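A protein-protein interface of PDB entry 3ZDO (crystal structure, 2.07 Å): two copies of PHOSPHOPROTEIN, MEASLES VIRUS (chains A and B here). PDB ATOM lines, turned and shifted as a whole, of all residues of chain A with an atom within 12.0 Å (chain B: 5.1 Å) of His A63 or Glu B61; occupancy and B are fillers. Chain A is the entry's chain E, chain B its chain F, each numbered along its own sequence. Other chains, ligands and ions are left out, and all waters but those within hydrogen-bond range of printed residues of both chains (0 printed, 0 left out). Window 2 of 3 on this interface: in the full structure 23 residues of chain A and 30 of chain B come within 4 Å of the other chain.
OG of Ser B65 sits at hydrogen-bond distance from OE2 of Glu B61.
Leu A60 touches its own counterpart, Leu B60. Leu A60 touches Glu B61, but with the chains exchanged Glu A61 does not touch Leu B60 (9.1 Å). His A63 touches Glu B61, but with the chains exchanged Glu A61 does not touch His B63 (11.5 Å). His A63 touches Leu B64, but with the chains exchanged Leu A64 does not touch His B63 (8.9 Å).
Of chain B, only Glu B61 (2.8 Å), Leu B64 (3.8 Å) and Met B68 (3.4 Å) come within 4 Å of His A63. Printed residues of chain A within 4 Å of Glu B61: Leu A60 (3.6 Å) and His A63 (2.8 Å). No residue of chain A comes within 4 Å of Ser B58. No residue of chain A comes within 4 Å of Thr B59. Gly B62 touches none of the printed residues of chain A. No residue of chain A comes within 4 Å of Ser B65. Of the printed residues of chain A, Met B68 touches His A63 and Ile A67. Printed residues of chain A within 4 Å of Leu B60: Leu A60 (3.8 Å). Of the printed residues of chain A, Leu B64 touches Leu A60 and His A63. Of the printed residues of chain B, Ile A67 touches Met B68. Printed residues of chain B within 4 Å of Ser A56: Ile B57 (3.8 Å). Gln A53 touches none of the printed residues of chain B. Leu A64 touches none of the printed residues of chain B. The nearest residue of chain B that does not touch His A63 is Ser B65 (4.3 Å). The nearest printed residue of chain A that does not touch Glu B61 is Thr A59 (4.1 Å).
ND1 of His A63 lies close to OE2 of Glu B61 (3.5 Å).
Ile B57 touches Ser A56. Leu B60 touches Leu A60 (CD2 to CD2, 3.8 Å). Glu B61 touches Leu A60. Leu A60 touches Leu B64. Leu B64 touches His A63. His A63 touches Met B68. Ile A67 touches Met B68.
Hydrophobic or aromatic side chains of chain B within 4 Å of the printed part of chain A: Ile B57, Leu B60, Leu B64 and Met B68. Among the printed residues, no Asp or Glu carboxylate lies within 4 Å of a Lys or Arg side-chain nitrogen of the other chain.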
ATOM      1  N   ARG A  52      33.627 -30.219  -7.508  1.00  0.00           N
ATOM      2  CA  ARG A  52      32.706 -29.114  -7.178  1.00  0.00           C
ATOM      3  C   ARG A  52      31.271 -29.363  -7.717  1.00  0.00           C
ATOM      4  O   ARG A  52      30.281 -29.101  -7.014  1.00  0.00           O
ATOM      5  CB  ARG A  52      33.211 -27.763  -7.706  1.00  0.00           C
ATOM      6  CG  ARG A  52      34.489 -27.223  -7.048  1.00  0.00           C
ATOM      7  CD  ARG A  52      34.621 -25.712  -7.242  1.00  0.00           C
ATOM      8  NE  ARG A  52      35.800 -25.172  -6.557  1.00  0.00           N
ATOM      9  CZ  ARG A  52      35.813 -24.730  -5.300  1.00  0.00           C
ATOM     10  NH1 ARG A  52      34.703 -24.744  -4.571  1.00  0.00           N
ATOM     11  NH2 ARG A  52      36.942 -24.266  -4.765  1.00  0.00           N
ATOM     12  N   GLN A  53      31.150 -29.872  -8.948  1.00  0.00           N
ATOM     13  CA  GLN A  53      29.831 -30.250  -9.432  1.00  0.00           C
ATOM     14  C   GLN A  53      29.099 -31.319  -8.598  1.00  0.00           C
ATOM     15  O   GLN A  53      27.888 -31.229  -8.419  1.00  0.00           O
ATOM     16  CB  GLN A  53      29.854 -30.688 -10.882  1.00  0.00           C
ATOM     17  CG  GLN A  53      28.455 -30.809 -11.465  1.00  0.00           C
ATOM     18  CD  GLN A  53      28.469 -30.875 -12.981  1.00  0.00           C
ATOM     19  OE1 GLN A  53      27.752 -31.676 -13.587  1.00  0.00           O
ATOM     20  NE2 GLN A  53      29.305 -30.071 -13.593  1.00  0.00           N
ATOM     21  N   ASN A  54      29.834 -32.361  -8.195  1.00  0.00           N
ATOM     22  CA  ASN A  54      29.288 -33.414  -7.350  1.00  0.00           C
ATOM     23  C   ASN A  54      28.679 -32.743  -6.109  1.00  0.00           C
ATOM     24  O   ASN A  54      27.489 -32.843  -5.881  1.00  0.00           O
ATOM     25  CB  ASN A  54      30.369 -34.456  -6.962  1.00  0.00           C
ATOM     26  CG  ASN A  54      30.850 -35.299  -8.146  1.00  0.00           C
ATOM     27  OD1 ASN A  54      31.961 -35.848  -8.131  1.00  0.00           O
ATOM     28  ND2 ASN A  54      30.027 -35.401  -9.172  1.00  0.00           N
ATOM     29  N   ILE A  55      29.501 -31.989  -5.376  1.00  0.00           N
ATOM     30  CA  ILE A  55      29.080 -31.254  -4.157  1.00  0.00           C
ATOM     31  C   ILE A  55      27.777 -30.487  -4.416  1.00  0.00           C
ATOM     32  O   ILE A  55      26.804 -30.618  -3.627  1.00  0.00           O
ATOM     33  CB  ILE A  55      30.169 -30.237  -3.659  1.00  0.00           C
ATOM     34  CG1 ILE A  55      31.444 -30.932  -3.147  1.00  0.00           C
ATOM     35  CG2 ILE A  55      29.598 -29.273  -2.612  1.00  0.00           C
ATOM     36  CD1 ILE A  55      31.190 -32.145  -2.272  1.00  0.00           C
ATOM     37  N   SER A  56      27.748 -29.728  -5.520  1.00  0.00           N
ATOM     38  CA  SER A  56      26.590 -28.880  -5.878  1.00  0.00           C
ATOM     39  C   SER A  56      25.329 -29.679  -6.229  1.00  0.00           C
ATOM     40  O   SER A  56      24.212 -29.204  -6.036  1.00  0.00           O
ATOM     41  CB  SER A  56      26.930 -27.895  -7.017  1.00  0.00           C
ATOM     42  OG  SER A  56      27.475 -26.677  -6.513  1.00  0.00           O
ATOM     43  N   ILE A  57      25.516 -30.900  -6.713  1.00  0.00           N
ATOM     44  CA  ILE A  57      24.412 -31.823  -6.946  1.00  0.00           C
ATOM     45  C   ILE A  57      23.868 -32.432  -5.627  1.00  0.00           C
ATOM     46  O   ILE A  57      22.670 -32.636  -5.492  1.00  0.00           O
ATOM     47  CB  ILE A  57      24.810 -32.915  -7.966  1.00  0.00           C
ATOM     48  CG1 ILE A  57      25.032 -32.268  -9.365  1.00  0.00           C
ATOM     49  CG2 ILE A  57      23.739 -33.997  -8.069  1.00  0.00           C
ATOM     50  CD1 ILE A  57      25.714 -33.174 -10.369  1.00  0.00           C
ATOM     51  N   SER A  58      24.760 -32.756  -4.690  1.00  0.00           N
ATOM     52  CA  SER A  58      24.386 -33.315  -3.390  1.00  0.00           C
ATOM     53  C   SER A  58      23.543 -32.343  -2.610  1.00  0.00           C
ATOM     54  O   SER A  58      22.620 -32.757  -1.904  1.00  0.00           O
ATOM     55  CB  SER A  58      25.637 -33.592  -2.537  1.00  0.00           C
ATOM     56  OG  SER A  58      26.290 -34.766  -2.946  1.00  0.00           O
ATOM     57  N   THR A  59      23.932 -31.055  -2.674  1.00  0.00           N
ATOM     58  CA  THR A  59      23.153 -29.976  -2.132  1.00  0.00           C
ATOM     59  C   THR A  59      21.719 -30.022  -2.648  1.00  0.00           C
ATOM     60  O   THR A  59      20.761 -30.013  -1.852  1.00  0.00           O
ATOM     61  CB  THR A  59      23.796 -28.601  -2.424  1.00  0.00           C
ATOM     62  OG1 THR A  59      25.134 -28.568  -1.887  1.00  0.00           O
ATOM     63  CG2 THR A  59      22.986 -27.509  -1.761  1.00  0.00           C
ATOM     64  N   LEU A  60      21.576 -30.103  -3.970  1.00  0.00           N
ATOM     65  CA  LEU A  60      20.266 -30.135  -4.623  1.00  0.00           C
ATOM     66  C   LEU A  60      19.406 -31.322  -4.162  1.00  0.00           C
ATOM     67  O   LEU A  60      18.223 -31.136  -3.888  1.00  0.00           O
ATOM     68  CB  LEU A  60      20.417 -30.132  -6.155  1.00  0.00           C
ATOM     69  CG  LEU A  60      19.423 -29.304  -6.975  1.00  0.00           C
ATOM     70  CD1 LEU A  60      19.627 -27.828  -6.697  1.00  0.00           C
ATOM     71  CD2 LEU A  60      19.595 -29.556  -8.464  1.00  0.00           C
ATOM     72  N   GLU A  61      20.011 -32.513  -4.047  1.00  0.00           N
ATOM     73  CA  GLU A  61      19.293 -33.739  -3.580  1.00  0.00           C
ATOM     74  C   GLU A  61      18.907 -33.572  -2.105  1.00  0.00           C
ATOM     75  O   GLU A  61      17.831 -33.985  -1.689  1.00  0.00           O
ATOM     76  CB  GLU A  61      20.157 -35.029  -3.747  1.00  0.00           C
ATOM     77  CG  GLU A  61      20.892 -35.175  -5.082  1.00  0.00           C
ATOM     78  CD  GLU A  61      21.852 -36.375  -5.159  1.00  0.00           C
ATOM     79  OE1 GLU A  61      22.898 -36.368  -4.460  1.00  0.00           O
ATOM     80  OE2 GLU A  61      21.581 -37.317  -5.956  1.00  0.00           O
ATOM     81  N   GLY A  62      19.802 -32.938  -1.340  1.00  0.00           N
ATOM     82  CA  GLY A  62      19.576 -32.609   0.072  1.00  0.00           C
ATOM     83  C   GLY A  62      18.329 -31.748   0.197  1.00  0.00           C
ATOM     84  O   GLY A  62      17.460 -31.993   1.062  1.00  0.00           O
ATOM     85  N   HIS A  63      18.226 -30.754  -0.688  1.00  0.00           N
ATOM     86  CA  HIS A  63      17.041 -29.902  -0.748  1.00  0.00           C
ATOM     87  C   HIS A  63      15.783 -30.649  -1.185  1.00  0.00           C
ATOM     88  O   HIS A  63      14.729 -30.480  -0.565  1.00  0.00           O
ATOM     89  CB  HIS A  63      17.259 -28.642  -1.604  1.00  0.00           C
ATOM     90  CG  HIS A  63      18.222 -27.659  -0.999  1.00  0.00           C
ATOM     91  ND1 HIS A  63      18.801 -26.635  -1.724  1.00  0.00           N
ATOM     92  CD2 HIS A  63      18.723 -27.558   0.256  1.00  0.00           C
ATOM     93  CE1 HIS A  63      19.606 -25.941  -0.938  1.00  0.00           C
ATOM     94  NE2 HIS A  63      19.579 -26.483   0.268  1.00  0.00           N
ATOM     95  N   LEU A  64      15.861 -31.441  -2.253  1.00  0.00           N
ATOM     96  CA  LEU A  64      14.702 -32.274  -2.584  1.00  0.00           C
ATOM     97  C   LEU A  64      14.361 -33.240  -1.425  1.00  0.00           C
ATOM     98  O   LEU A  64      13.188 -33.497  -1.155  1.00  0.00           O
ATOM     99  CB  LEU A  64      14.854 -32.993  -3.932  1.00  0.00           C
ATOM    100  CG  LEU A  64      14.744 -32.154  -5.220  1.00  0.00           C
ATOM    101  CD1 LEU A  64      14.645 -33.054  -6.435  1.00  0.00           C
ATOM    102  CD2 LEU A  64      13.551 -31.217  -5.210  1.00  0.00           C
ATOM    103  N   SER A  65      15.375 -33.708  -0.692  1.00  0.00           N
ATOM    104  CA  SER A  65      15.119 -34.542   0.487  1.00  0.00           C
ATOM    105  C   SER A  65      14.304 -33.821   1.558  1.00  0.00           C
ATOM    106  O   SER A  65      13.316 -34.354   2.025  1.00  0.00           O
ATOM    107  CB  SER A  65      16.405 -35.111   1.076  1.00  0.00           C
ATOM    108  OG  SER A  65      16.700 -36.379   0.514  1.00  0.00           O
ATOM    109  N   SER A  66      14.734 -32.620   1.938  1.00  0.00           N
ATOM    110  CA  SER A  66      14.031 -31.758   2.891  1.00  0.00           C
ATOM    111  C   SER A  66      12.561 -31.485   2.545  1.00  0.00           C
ATOM    112  O   SER A  66      11.698 -31.515   3.420  1.00  0.00           O
ATOM    113  CB  SER A  66      14.757 -30.416   3.019  1.00  0.00           C
ATOM    114  OG  SER A  66      15.695 -30.440   4.073  1.00  0.00           O
ATOM    115  N   ILE A  67      12.299 -31.154   1.286  1.00  0.00           N
ATOM    116  CA  ILE A  67      10.940 -30.998   0.789  1.00  0.00           C
ATOM    117  C   ILE A  67      10.156 -32.307   0.865  1.00  0.00           C
ATOM    118  O   ILE A  67       8.923 -32.286   0.982  1.00  0.00           O
ATOM    119  CB  ILE A  67      10.945 -30.473  -0.657  1.00  0.00           C
ATOM    120  CG1 ILE A  67      11.469 -29.027  -0.679  1.00  0.00           C
ATOM    121  CG2 ILE A  67       9.558 -30.592  -1.302  1.00  0.00           C
ATOM    122  CD1 ILE A  67      12.091 -28.626  -2.002  1.00  0.00           C
ATOM    123  N   ILE B  57      24.191 -25.059 -12.339  1.00  0.00           N
ATOM    124  CA  ILE B  57      23.672 -25.835 -11.179  1.00  0.00           C
ATOM    125  C   ILE B  57      23.270 -24.861 -10.088  1.00  0.00           C
ATOM    126  O   ILE B  57      22.298 -25.087  -9.385  1.00  0.00           O
ATOM    127  CB  ILE B  57      24.672 -26.888 -10.578  1.00  0.00           C
ATOM    128  CG1 ILE B  57      25.297 -27.778 -11.668  1.00  0.00           C
ATOM    129  CG2 ILE B  57      23.991 -27.809  -9.551  1.00  0.00           C
ATOM    130  CD1 ILE B  57      24.306 -28.408 -12.614  1.00  0.00           C
ATOM    131  N   SER B  58      24.019 -23.764  -9.976  1.00  0.00           N
ATOM    132  CA  SER B  58      23.778 -22.728  -8.966  1.00  0.00           C
ATOM    133  C   SER B  58      22.491 -21.956  -9.173  1.00  0.00           C
ATOM    134  O   SER B  58      21.754 -21.667  -8.224  1.00  0.00           O
ATOM    135  CB  SER B  58      24.946 -21.758  -8.924  1.00  0.00           C
ATOM    136  OG  SER B  58      25.867 -22.188  -7.952  1.00  0.00           O
ATOM    137  N   THR B  59      22.192 -21.628 -10.415  1.00  0.00           N
ATOM    138  CA  THR B  59      20.871 -21.113 -10.681  1.00  0.00           C
ATOM    139  C   THR B  59      19.827 -22.082 -10.120  1.00  0.00           C
ATOM    140  O   THR B  59      19.015 -21.671  -9.281  1.00  0.00           O
ATOM    141  CB  THR B  59      20.647 -20.807 -12.161  1.00  0.00           C
ATOM    142  OG1 THR B  59      21.820 -20.183 -12.680  1.00  0.00           O
ATOM    143  CG2 THR B  59      19.456 -19.867 -12.329  1.00  0.00           C
ATOM    144  N   LEU B  60      19.899 -23.371 -10.503  1.00  0.00           N
ATOM    145  CA  LEU B  60      18.934 -24.386  -9.999  1.00  0.00           C
ATOM    146  C   LEU B  60      18.787 -24.299  -8.520  1.00  0.00           C
ATOM    147  O   LEU B  60      17.674 -24.324  -7.990  1.00  0.00           O
ATOM    148  CB  LEU B  60      19.407 -25.830 -10.283  1.00  0.00           C
ATOM    149  CG  LEU B  60      19.076 -26.579 -11.572  1.00  0.00           C
ATOM    150  CD1 LEU B  60      19.118 -25.653 -12.765  1.00  0.00           C
ATOM    151  CD2 LEU B  60      20.068 -27.716 -11.757  1.00  0.00           C
ATOM    152  N   GLU B  61      19.928 -24.318  -7.841  1.00  0.00           N
ATOM    153  CA  GLU B  61      19.940 -24.293  -6.393  1.00  0.00           C
ATOM    154  C   GLU B  61      19.245 -23.012  -5.861  1.00  0.00           C
ATOM    155  O   GLU B  61      18.483 -23.059  -4.868  1.00  0.00           O
ATOM    156  CB  GLU B  61      21.386 -24.436  -5.850  1.00  0.00           C
ATOM    157  CG  GLU B  61      21.430 -24.814  -4.362  1.00  0.00           C
ATOM    158  CD  GLU B  61      21.212 -23.607  -3.451  1.00  0.00           C
ATOM    159  OE1 GLU B  61      21.649 -22.497  -3.841  1.00  0.00           O
ATOM    160  OE2 GLU B  61      20.583 -23.746  -2.362  1.00  0.00           O
ATOM    161  N   GLY B  62      19.529 -21.882  -6.510  1.00  0.00           N
ATOM    162  CA  GLY B  62      18.830 -20.611  -6.239  1.00  0.00           C
ATOM    163  C   GLY B  62      17.310 -20.694  -6.289  1.00  0.00           C
ATOM    164  O   GLY B  62      16.623 -20.260  -5.348  1.00  0.00           O
ATOM    165  N   HIS B  63      16.775 -21.275  -7.361  1.00  0.00           N
ATOM    166  CA  HIS B  63      15.330 -21.438  -7.465  1.00  0.00           C
ATOM    167  C   HIS B  63      14.853 -22.484  -6.476  1.00  0.00           C
ATOM    168  O   HIS B  63      13.765 -22.354  -5.910  1.00  0.00           O
ATOM    169  CB  HIS B  63      14.886 -21.822  -8.871  1.00  0.00           C
ATOM    170  CG  HIS B  63      15.388 -20.910  -9.949  1.00  0.00           C
ATOM    171  ND1 HIS B  63      15.475 -21.306 -11.270  1.00  0.00           N
ATOM    172  CD2 HIS B  63      15.806 -19.619  -9.917  1.00  0.00           C
ATOM    173  CE1 HIS B  63      15.930 -20.303 -12.002  1.00  0.00           C
ATOM    174  NE2 HIS B  63      16.139 -19.268 -11.206  1.00  0.00           N
ATOM    175  N   LEU B  64      15.663 -23.519  -6.252  1.00  0.00           N
ATOM    176  CA  LEU B  64      15.287 -24.525  -5.287  1.00  0.00           C
ATOM    177  C   LEU B  64      15.141 -23.982  -3.865  1.00  0.00           C
ATOM    178  O   LEU B  64      14.219 -24.384  -3.159  1.00  0.00           O
ATOM    179  CB  LEU B  64      16.244 -25.694  -5.318  1.00  0.00           C
ATOM    180  CG  LEU B  64      15.660 -27.024  -5.743  1.00  0.00           C
ATOM    181  CD1 LEU B  64      16.630 -28.090  -5.280  1.00  0.00           C
ATOM    182  CD2 LEU B  64      14.282 -27.254  -5.132  1.00  0.00           C
ATOM    183  N   SER B  65      16.038 -23.070  -3.463  1.00  0.00           N
ATOM    184  CA  SER B  65      15.901 -22.288  -2.203  1.00  0.00           C
ATOM    185  C   SER B  65      14.592 -21.479  -2.096  1.00  0.00           C
ATOM    186  O   SER B  65      13.951 -21.488  -1.062  1.00  0.00           O
ATOM    187  CB  SER B  65      17.109 -21.344  -1.975  1.00  0.00           C
ATOM    188  OG  SER B  65      18.348 -22.015  -2.124  1.00  0.00           O
ATOM    189  N   MET B  68      11.830 -23.932  -1.234  1.00  0.00           N
ATOM    190  CA  MET B  68      11.899 -24.426   0.147  1.00  0.00           C
ATOM    191  C   MET B  68      11.304 -23.469   1.188  1.00  0.00           C
ATOM    192  O   MET B  68      10.664 -23.917   2.151  1.00  0.00           O
ATOM    193  CB  MET B  68      13.322 -24.813   0.530  1.00  0.00           C
ATOM    194  CG  MET B  68      13.769 -26.162  -0.006  1.00  0.00           C
ATOM    195  SD  MET B  68      15.070 -26.866   1.025  1.00  0.00           S
ATOM    196  CE  MET B  68      16.176 -25.452   1.172  1.00  0.00           C
